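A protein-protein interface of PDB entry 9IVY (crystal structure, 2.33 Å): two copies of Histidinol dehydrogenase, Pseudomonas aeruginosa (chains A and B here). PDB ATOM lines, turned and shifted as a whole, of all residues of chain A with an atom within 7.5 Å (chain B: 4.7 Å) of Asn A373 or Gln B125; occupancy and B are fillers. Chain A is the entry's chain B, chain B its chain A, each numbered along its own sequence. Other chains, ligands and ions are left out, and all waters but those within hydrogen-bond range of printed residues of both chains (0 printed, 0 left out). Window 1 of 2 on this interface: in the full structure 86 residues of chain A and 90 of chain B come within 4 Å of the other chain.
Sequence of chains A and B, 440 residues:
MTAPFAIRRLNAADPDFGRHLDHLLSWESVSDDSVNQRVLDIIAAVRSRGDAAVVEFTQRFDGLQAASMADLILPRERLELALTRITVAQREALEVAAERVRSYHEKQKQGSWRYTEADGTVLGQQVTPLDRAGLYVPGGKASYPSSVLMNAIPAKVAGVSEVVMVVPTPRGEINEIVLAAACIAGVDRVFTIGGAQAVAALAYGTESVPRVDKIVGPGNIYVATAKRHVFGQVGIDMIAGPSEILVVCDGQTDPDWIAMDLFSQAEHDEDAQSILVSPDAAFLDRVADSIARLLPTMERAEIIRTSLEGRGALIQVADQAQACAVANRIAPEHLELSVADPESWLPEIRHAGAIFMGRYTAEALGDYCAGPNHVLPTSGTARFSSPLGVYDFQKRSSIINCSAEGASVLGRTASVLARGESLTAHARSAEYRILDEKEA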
ATOM      1  N   TYR A 104      18.158 -17.394   9.401  1.00  0.00           N
ATOM      2  CA  TYR A 104      18.583 -17.650  10.775  1.00  0.00           C
ATOM      3  C   TYR A 104      19.963 -18.301  10.814  1.00  0.00           C
ATOM      4  O   TYR A 104      20.868 -17.835  11.516  1.00  0.00           O
ATOM      5  CB  TYR A 104      17.532 -18.526  11.463  1.00  0.00           C
ATOM      6  CG  TYR A 104      17.903 -19.071  12.824  1.00  0.00           C
ATOM      7  CD1 TYR A 104      17.631 -18.353  13.982  1.00  0.00           C
ATOM      8  CD2 TYR A 104      18.497 -20.322  12.953  1.00  0.00           C
ATOM      9  CE1 TYR A 104      17.957 -18.860  15.232  1.00  0.00           C
ATOM     10  CE2 TYR A 104      18.831 -20.834  14.193  1.00  0.00           C
ATOM     11  CZ  TYR A 104      18.559 -20.102  15.328  1.00  0.00           C
ATOM     12  OH  TYR A 104      18.893 -20.619  16.557  1.00  0.00           O
ATOM     13  N   HIS A 105      20.149 -19.378  10.049  1.00  0.00           N
ATOM     14  CA  HIS A 105      21.420 -20.094  10.101  1.00  0.00           C
ATOM     15  C   HIS A 105      22.572 -19.250   9.574  1.00  0.00           C
ATOM     16  O   HIS A 105      23.717 -19.439  10.002  1.00  0.00           O
ATOM     17  CB  HIS A 105      21.313 -21.401   9.322  1.00  0.00           C
ATOM     18  CG  HIS A 105      20.488 -22.442  10.009  1.00  0.00           C
ATOM     19  ND1 HIS A 105      20.633 -22.740  11.347  1.00  0.00           N
ATOM     20  CD2 HIS A 105      19.503 -23.247   9.547  1.00  0.00           C
ATOM     21  CE1 HIS A 105      19.778 -23.691  11.678  1.00  0.00           C
ATOM     22  NE2 HIS A 105      19.081 -24.017  10.604  1.00  0.00           N
ATOM     23  N   GLN A 108      23.851 -17.231  12.496  1.00  0.00           N
ATOM     24  CA  GLN A 108      24.546 -17.994  13.527  1.00  0.00           C
ATOM     25  C   GLN A 108      25.891 -18.552  13.078  1.00  0.00           C
ATOM     26  O   GLN A 108      26.698 -18.937  13.933  1.00  0.00           O
ATOM     27  CB  GLN A 108      23.667 -19.147  14.010  1.00  0.00           C
ATOM     28  CG  GLN A 108      22.322 -18.695  14.543  1.00  0.00           C
ATOM     29  CD  GLN A 108      22.024 -19.265  15.910  1.00  0.00           C
ATOM     30  OE1 GLN A 108      21.952 -20.481  16.090  1.00  0.00           O
ATOM     31  NE2 GLN A 108      21.863 -18.385  16.888  1.00  0.00           N
ATOM     32  N   LEU A 346       5.864 -23.769  34.487  1.00  0.00           N
ATOM     33  CA  LEU A 346       7.178 -24.281  34.100  1.00  0.00           C
ATOM     34  C   LEU A 346       8.108 -24.599  35.270  1.00  0.00           C
ATOM     35  O   LEU A 346       8.839 -25.600  35.172  1.00  0.00           O
ATOM     36  CB  LEU A 346       7.849 -23.291  33.141  1.00  0.00           C
ATOM     37  CG  LEU A 346       8.931 -23.882  32.236  1.00  0.00           C
ATOM     38  CD1 LEU A 346       8.347 -24.981  31.384  1.00  0.00           C
ATOM     39  CD2 LEU A 346       9.535 -22.796  31.364  1.00  0.00           C
ATOM     40  N   GLY A 353      11.419 -31.727  27.138  1.00  0.00           N
ATOM     41  CA  GLY A 353      12.235 -31.134  26.098  1.00  0.00           C
ATOM     42  C   GLY A 353      11.645 -29.848  25.556  1.00  0.00           C
ATOM     43  O   GLY A 353      11.742 -28.798  26.197  1.00  0.00           O
ATOM     44  N   ALA A 354      11.029 -29.921  24.379  1.00  0.00           N
ATOM     45  CA  ALA A 354      10.417 -28.756  23.755  1.00  0.00           C
ATOM     46  C   ALA A 354       9.064 -28.459  24.382  1.00  0.00           C
ATOM     47  O   ALA A 354       8.270 -29.368  24.642  1.00  0.00           O
ATOM     48  CB  ALA A 354      10.245 -28.987  22.259  1.00  0.00           C
ATOM     49  N   ALA A 370       9.710 -24.902  13.262  1.00  0.00           N
ATOM     50  CA  ALA A 370      10.720 -24.907  14.328  1.00  0.00           C
ATOM     51  C   ALA A 370      11.429 -26.262  14.315  1.00  0.00           C
ATOM     52  O   ALA A 370      11.048 -27.186  15.040  1.00  0.00           O
ATOM     53  CB  ALA A 370      10.090 -24.618  15.685  1.00  0.00           C
ATOM     54  N   GLY A 371      12.476 -26.366  13.505  1.00  0.00           N
ATOM     55  CA  GLY A 371      13.226 -27.593  13.375  1.00  0.00           C
ATOM     56  C   GLY A 371      14.522 -27.686  14.165  1.00  0.00           C
ATOM     57  O   GLY A 371      14.797 -28.713  14.796  1.00  0.00           O
ATOM     58  N   PRO A 372      15.361 -26.644  14.136  1.00  0.00           N
ATOM     59  CA  PRO A 372      16.637 -26.725  14.868  1.00  0.00           C
ATOM     60  C   PRO A 372      16.409 -26.591  16.367  1.00  0.00           C
ATOM     61  O   PRO A 372      15.846 -25.598  16.832  1.00  0.00           O
ATOM     62  CB  PRO A 372      17.441 -25.543  14.311  1.00  0.00           C
ATOM     63  CG  PRO A 372      16.412 -24.552  13.908  1.00  0.00           C
ATOM     64  CD  PRO A 372      15.220 -25.349  13.437  1.00  0.00           C
ATOM     65  N   ASN A 373      16.822 -27.618  17.117  1.00  0.00           N
ATOM     66  CA  ASN A 373      16.728 -27.673  18.576  1.00  0.00           C
ATOM     67  C   ASN A 373      15.347 -27.296  19.105  1.00  0.00           C
ATOM     68  O   ASN A 373      15.181 -27.076  20.310  1.00  0.00           O
ATOM     69  CB  ASN A 373      17.815 -26.788  19.215  1.00  0.00           C
ATOM     70  CG  ASN A 373      17.491 -25.295  19.178  1.00  0.00           C
ATOM     71  OD1 ASN A 373      16.631 -24.810  19.914  1.00  0.00           O
ATOM     72  ND2 ASN A 373      18.199 -24.559  18.325  1.00  0.00           N
ATOM     73  N   HIS A 374      14.355 -27.247  18.211  1.00  0.00           N
ATOM     74  CA  HIS A 374      12.982 -26.844  18.494  1.00  0.00           C
ATOM     75  C   HIS A 374      12.836 -25.348  18.747  1.00  0.00           C
ATOM     76  O   HIS A 374      11.818 -24.917  19.293  1.00  0.00           O
ATOM     77  CB  HIS A 374      12.387 -27.622  19.675  1.00  0.00           C
ATOM     78  CG  HIS A 374      11.813 -28.947  19.295  1.00  0.00           C
ATOM     79  ND1 HIS A 374      12.422 -30.140  19.622  1.00  0.00           N
ATOM     80  CD2 HIS A 374      10.683 -29.271  18.622  1.00  0.00           C
ATOM     81  CE1 HIS A 374      11.692 -31.142  19.162  1.00  0.00           C
ATOM     82  NE2 HIS A 374      10.631 -30.642  18.553  1.00  0.00           N
ATOM     83  N   VAL A 375      13.818 -24.529  18.380  1.00  0.00           N
ATOM     84  CA  VAL A 375      13.649 -23.083  18.476  1.00  0.00           C
ATOM     85  C   VAL A 375      13.124 -22.565  17.147  1.00  0.00           C
ATOM     86  O   VAL A 375      13.459 -23.087  16.075  1.00  0.00           O
ATOM     87  CB  VAL A 375      14.959 -22.377  18.881  1.00  0.00           C
ATOM     88  CG1 VAL A 375      15.918 -22.273  17.702  1.00  0.00           C
ATOM     89  CG2 VAL A 375      14.659 -20.993  19.462  1.00  0.00           C
ATOM     90  N   LEU A 376      12.274 -21.555  17.218  1.00  0.00           N
ATOM     91  CA  LEU A 376      11.745 -20.940  16.010  1.00  0.00           C
ATOM     92  C   LEU A 376      12.790 -20.008  15.407  1.00  0.00           C
ATOM     93  O   LEU A 376      13.291 -19.117  16.099  1.00  0.00           O
ATOM     94  CB  LEU A 376      10.467 -20.173  16.317  1.00  0.00           C
ATOM     95  CG  LEU A 376       9.525 -20.019  15.124  1.00  0.00           C
ATOM     96  CD1 LEU A 376       8.638 -21.244  14.988  1.00  0.00           C
ATOM     97  CD2 LEU A 376       8.697 -18.745  15.254  1.00  0.00           C
ATOM     98  N   THR A 381      15.944 -14.622  17.733  1.00  0.00           N
ATOM     99  CA  THR A 381      16.419 -15.876  18.307  1.00  0.00           C
ATOM    100  C   THR A 381      17.849 -16.196  17.885  1.00  0.00           C
ATOM    101  O   THR A 381      18.518 -16.992  18.556  1.00  0.00           O
ATOM    102  CB  THR A 381      15.484 -17.030  17.925  1.00  0.00           C
ATOM    103  OG1 THR A 381      15.373 -17.126  16.501  1.00  0.00           O
ATOM    104  CG2 THR A 381      14.114 -16.792  18.500  1.00  0.00           C
ATOM    105  N   PHE A 384      21.178 -15.854  20.134  1.00  0.00           N
ATOM    106  CA  PHE A 384      21.417 -16.850  21.175  1.00  0.00           C
ATOM    107  C   PHE A 384      21.994 -18.105  20.527  1.00  0.00           C
ATOM    108  O   PHE A 384      21.300 -18.802  19.778  1.00  0.00           O
ATOM    109  CB  PHE A 384      20.127 -17.134  21.940  1.00  0.00           C
ATOM    110  CG  PHE A 384      19.448 -15.887  22.443  1.00  0.00           C
ATOM    111  CD1 PHE A 384      18.602 -15.154  21.620  1.00  0.00           C
ATOM    112  CD2 PHE A 384      19.684 -15.427  23.731  1.00  0.00           C
ATOM    113  CE1 PHE A 384      17.996 -13.994  22.076  1.00  0.00           C
ATOM    114  CE2 PHE A 384      19.077 -14.268  24.193  1.00  0.00           C
ATOM    115  CZ  PHE A 384      18.232 -13.552  23.365  1.00  0.00           C
ATOM    116  N   SER A 385      23.260 -18.387  20.830  1.00  0.00           N
ATOM    117  CA  SER A 385      24.047 -19.376  20.109  1.00  0.00           C
ATOM    118  C   SER A 385      23.622 -20.796  20.467  1.00  0.00           C
ATOM    119  O   SER A 385      23.065 -21.065  21.535  1.00  0.00           O
ATOM    120  CB  SER A 385      25.537 -19.188  20.402  1.00  0.00           C
ATOM    121  OG  SER A 385      26.250 -20.400  20.225  1.00  0.00           O
ATOM    122  N   SER A 386      23.911 -21.717  19.546  1.00  0.00           N
ATOM    123  CA  SER A 386      23.544 -23.109  19.698  1.00  0.00           C
ATOM    124  C   SER A 386      24.585 -23.988  19.021  1.00  0.00           C
ATOM    125  O   SER A 386      25.007 -23.679  17.896  1.00  0.00           O
ATOM    126  CB  SER A 386      22.160 -23.393  19.102  1.00  0.00           C
ATOM    127  OG  SER A 386      22.212 -23.438  17.684  1.00  0.00           O
ATOM    128  N   PRO A 387      25.021 -25.071  19.671  1.00  0.00           N
ATOM    129  CA  PRO A 387      25.817 -26.081  18.964  1.00  0.00           C
ATOM    130  C   PRO A 387      25.013 -26.845  17.938  1.00  0.00           C
ATOM    131  O   PRO A 387      25.594 -27.585  17.135  1.00  0.00           O
ATOM    132  CB  PRO A 387      26.288 -27.005  20.090  1.00  0.00           C
ATOM    133  CG  PRO A 387      25.187 -26.923  21.077  1.00  0.00           C
ATOM    134  CD  PRO A 387      24.737 -25.478  21.055  1.00  0.00           C
ATOM    135  N   LEU A 388      23.694 -26.699  17.952  1.00  0.00           N
ATOM    136  CA  LEU A 388      22.837 -27.290  16.944  1.00  0.00           C
ATOM    137  C   LEU A 388      22.774 -26.381  15.717  1.00  0.00           C
ATOM    138  O   LEU A 388      23.182 -25.216  15.745  1.00  0.00           O
ATOM    139  CB  LEU A 388      21.454 -27.544  17.538  1.00  0.00           C
ATOM    140  CG  LEU A 388      21.562 -28.540  18.697  1.00  0.00           C
ATOM    141  CD1 LEU A 388      20.931 -28.002  19.964  1.00  0.00           C
ATOM    142  CD2 LEU A 388      20.947 -29.878  18.315  1.00  0.00           C
ATOM    143  N   GLY A 389      22.273 -26.932  14.623  1.00  0.00           N
ATOM    144  CA  GLY A 389      22.211 -26.168  13.388  1.00  0.00           C
ATOM    145  C   GLY A 389      23.547 -26.179  12.685  1.00  0.00           C
ATOM    146  O   GLY A 389      24.121 -27.244  12.440  1.00  0.00           O
ATOM    147  N   SER B 112      18.811 -19.006  31.260  1.00  0.00           N
ATOM    148  CA  SER B 112      17.527 -18.953  30.579  1.00  0.00           C
ATOM    149  C   SER B 112      17.307 -17.574  29.971  1.00  0.00           C
ATOM    150  O   SER B 112      17.762 -16.556  30.500  1.00  0.00           O
ATOM    151  CB  SER B 112      16.398 -19.291  31.549  1.00  0.00           C
ATOM    152  OG  SER B 112      16.719 -20.441  32.305  1.00  0.00           O
ATOM    153  N   TRP B 113      16.611 -17.545  28.838  1.00  0.00           N
ATOM    154  CA  TRP B 113      16.362 -16.291  28.141  1.00  0.00           C
ATOM    155  C   TRP B 113      14.987 -16.322  27.491  1.00  0.00           C
ATOM    156  O   TRP B 113      14.417 -17.386  27.233  1.00  0.00           O
ATOM    157  CB  TRP B 113      17.443 -16.008  27.088  1.00  0.00           C
ATOM    158  CG  TRP B 113      17.530 -17.027  25.988  1.00  0.00           C
ATOM    159  CD1 TRP B 113      18.254 -18.188  25.996  1.00  0.00           C
ATOM    160  CD2 TRP B 113      16.891 -16.965  24.706  1.00  0.00           C
ATOM    161  NE1 TRP B 113      18.101 -18.848  24.802  1.00  0.00           N
ATOM    162  CE2 TRP B 113      17.268 -18.117  23.993  1.00  0.00           C
ATOM    163  CE3 TRP B 113      16.036 -16.044  24.095  1.00  0.00           C
ATOM    164  CZ2 TRP B 113      16.814 -18.379  22.704  1.00  0.00           C
ATOM    165  CZ3 TRP B 113      15.591 -16.300  22.814  1.00  0.00           C
ATOM    166  CH2 TRP B 113      15.981 -17.457  22.132  1.00  0.00           C
ATOM    167  N   ARG B 114      14.460 -15.126  27.240  1.00  0.00           N
ATOM    168  CA  ARG B 114      13.217 -14.938  26.507  1.00  0.00           C
ATOM    169  C   ARG B 114      13.384 -13.749  25.577  1.00  0.00           C
ATOM    170  O   ARG B 114      14.030 -12.762  25.939  1.00  0.00           O
ATOM    171  CB  ARG B 114      12.029 -14.692  27.448  1.00  0.00           C
ATOM    172  CG  ARG B 114      11.731 -15.827  28.423  1.00  0.00           C
ATOM    173  CD  ARG B 114      10.941 -16.964  27.767  1.00  0.00           C
ATOM    174  NE  ARG B 114      10.574 -17.992  28.736  1.00  0.00           N
ATOM    175  CZ  ARG B 114      11.427 -18.841  29.296  1.00  0.00           C
ATOM    176  NH1 ARG B 114      12.708 -18.857  28.962  1.00  0.00           N
ATOM    177  NH2 ARG B 114      10.985 -19.694  30.216  1.00  0.00           N
ATOM    178  N   GLY B 124      12.291 -18.634  23.514  1.00  0.00           N
ATOM    179  CA  GLY B 124      13.394 -18.661  24.455  1.00  0.00           C
ATOM    180  C   GLY B 124      13.818 -20.074  24.791  1.00  0.00           C
ATOM    181  O   GLY B 124      13.470 -21.029  24.094  1.00  0.00           O
ATOM    182  N   GLN B 125      14.593 -20.176  25.870  1.00  0.00           N
ATOM    183  CA  GLN B 125      15.062 -21.446  26.402  1.00  0.00           C
ATOM    184  C   GLN B 125      15.069 -21.364  27.918  1.00  0.00           C
ATOM    185  O   GLN B 125      15.468 -20.347  28.490  1.00  0.00           O
ATOM    186  CB  GLN B 125      16.469 -21.792  25.902  1.00  0.00           C
ATOM    187  CG  GLN B 125      16.547 -22.214  24.453  1.00  0.00           C
ATOM    188  CD  GLN B 125      17.977 -22.448  24.006  1.00  0.00           C
ATOM    189  OE1 GLN B 125      18.867 -21.650  24.296  1.00  0.00           O
ATOM    190  NE2 GLN B 125      18.208 -23.548  23.296  1.00  0.00           N
ATOM    191  N   GLN B 126      14.615 -22.429  28.565  1.00  0.00           N
ATOM    192  CA  GLN B 126      14.732 -22.565  30.008  1.00  0.00           C
ATOM    193  C   GLN B 126      15.955 -23.431  30.281  1.00  0.00           C
ATOM    194  O   GLN B 126      15.981 -24.615  29.924  1.00  0.00           O
ATOM    195  CB  GLN B 126      13.468 -23.163  30.619  1.00  0.00           C
ATOM    196  CG  GLN B 126      13.413 -23.047  32.131  1.00  0.00           C
ATOM    197  CD  GLN B 126      13.296 -21.611  32.601  1.00  0.00           C
ATOM    198  OE1 GLN B 126      12.972 -20.714  31.823  1.00  0.00           O
ATOM    199  NE2 GLN B 126      13.567 -21.386  33.880  1.00  0.00           N
ATOM    200  N   VAL B 127      16.971 -22.828  30.890  1.00  0.00           N
ATOM    201  CA  VAL B 127      18.256 -23.474  31.114  1.00  0.00           C
ATOM    202  C   VAL B 127      18.339 -23.907  32.569  1.00  0.00           C
ATOM    203  O   VAL B 127      18.133 -23.098  33.482  1.00  0.00           O
ATOM    204  CB  VAL B 127      19.412 -22.534  30.745  1.00  0.00           C
ATOM    205  CG1 VAL B 127      20.746 -23.240  30.937  1.00  0.00           C
ATOM    206  CG2 VAL B 127      19.237 -22.049  29.314  1.00  0.00           C
ATOM    207  N   ARG B 396      18.587 -27.823  28.283  1.00  0.00           N
ATOM    208  CA  ARG B 396      17.896 -26.732  27.618  1.00  0.00           C
ATOM    209  C   ARG B 396      16.539 -27.201  27.112  1.00  0.00           C
ATOM    210  O   ARG B 396      16.413 -28.294  26.552  1.00  0.00           O
ATOM    211  CB  ARG B 396      18.739 -26.173  26.465  1.00  0.00           C
ATOM    212  CG  ARG B 396      19.422 -24.860  26.814  1.00  0.00           C
ATOM    213  CD  ARG B 396      20.720 -24.666  26.054  1.00  0.00           C
ATOM    214  NE  ARG B 396      21.755 -24.057  26.885  1.00  0.00           N
ATOM    215  CZ  ARG B 396      21.929 -22.749  27.027  1.00  0.00           C
ATOM    216  NH1 ARG B 396      21.147 -21.875  26.409  1.00  0.00           N
ATOM    217  NH2 ARG B 396      22.910 -22.305  27.807  1.00  0.00           N
ATOM    218  N   SER B 397      15.527 -26.366  27.330  1.00  0.00           N
ATOM    219  CA  SER B 397      14.159 -26.623  26.900  1.00  0.00           C
ATOM    220  C   SER B 397      13.719 -25.470  26.012  1.00  0.00           C
ATOM    221  O   SER B 397      13.663 -24.324  26.467  1.00  0.00           O
ATOM    222  CB  SER B 397      13.222 -26.761  28.102  1.00  0.00           C
ATOM    223  OG  SER B 397      13.128 -28.105  28.533  1.00  0.00           O
ATOM    224  N   SER B 398      13.408 -25.767  24.757  1.00  0.00           N
ATOM    225  CA  SER B 398      12.960 -24.732  23.837  1.00  0.00           C
ATOM    226  C   SER B 398      11.522 -24.324  24.145  1.00  0.00           C
ATOM    227  O   SER B 398      10.672 -25.165  24.459  1.00  0.00           O
ATOM    228  CB  SER B 398      13.076 -25.214  22.394  1.00  0.00           C
ATOM    229  OG  SER B 398      12.940 -24.123  21.502  1.00  0.00           O
ATOM    230  N   ILE B 399      11.255 -23.024  24.051  1.00  0.00           N
ATOM    231  CA  ILE B 399       9.962 -22.442  24.398  1.00  0.00           C
ATOM    232  C   ILE B 399       9.444 -21.656  23.203  1.00  0.00           C
ATOM    233  O   ILE B 399      10.126 -20.752  22.707  1.00  0.00           O
ATOM    234  CB  ILE B 399      10.055 -21.530  25.632  1.00  0.00           C
ATOM    235  CG1 ILE B 399      10.223 -22.359  26.906  1.00  0.00           C
ATOM    236  CG2 ILE B 399       8.828 -20.624  25.727  1.00  0.00           C
ATOM    237  CD1 ILE B 399      11.566 -22.215  27.540  1.00  0.00           C
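The side-chain hydroxyl (OG) of Ser B397 lies within hydrogen-bond range of the backbone carbonyl oxygen (O) of Gly A353 (2.8 Å). The side-chain hydroxyl of Ser B398 is in hydrogen-bond range of the backbone carbonyl oxygen of His A374, at 2.6 Å. OG of Ser B398 sits at hydrogen-bond distance from N of Val A375 (3.3 Å).
OE1 of Gln B125 is in hydrogen-bond range of NE1 of Trp B113, 2.9 Å away. NH1 of Arg B114 is in hydrogen-bond range of O of Gln B125 (3.2 Å). NH2 of Arg B114 lies within hydrogen-bond range of OE1 of Gln B126 (2.8 Å). The backbone NH (N) of Gln B126 lies within hydrogen-bond range of the backbone carbonyl oxygen (O) of Ser B397. NE2 of Gln A108 lies within hydrogen-bond range of O of Phe A384, at 3.0 Å. The side-chain amide oxygen (OD1) of Asn A373 sits close to the backbone NH (N) of Val A375 (3.2 Å).
CD2 of Leu A346 touches NH2 of Arg B114, 3.6 Å away. CD2 of Leu A346 touches CG of Gln B126, 3.96 Å away. Ser B398 touches Gly A353. C of Ala A354 touches O of Ser B398, 3.7 Å away. OD1 of Asn A373 touches NE2 of Gln B125, at 3.9 Å. Ser B398 touches Asn A373 (CB to O, 3.5 Å). Phe A384 touches Trp B113 (CD2 to CD2, 3.3 Å).
Asn A373 touches two residues of chain B. Printed residues of chain A within 4 Å of Trp B113: Phe A384 (3.3 Å). Of the printed residues of chain B, Ala A354 touches Ser B398 (3.7 Å). Of the printed residues of chain B, Phe A384 touches Trp B113. The nearest residue of chain A that does not touch Gln B125 is Ser A385 (5.1 Å). The nearest printed residue of chain A that does not touch Ser B398 is Leu A376 (5.0 Å).
Of the 20 printed residues of chain A, 7 touch a printed residue of chain B. Along chain A the printed residues that touch a printed residue of chain B span positions 346 to 384. Among the printed residues, 10 pairs touch across the chains. Among the printed residues, no Asp or Glu carboxylate lies within 4 Å of a Lys or Arg side-chain nitrogen of the other chain.
No position is printed for both chains.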
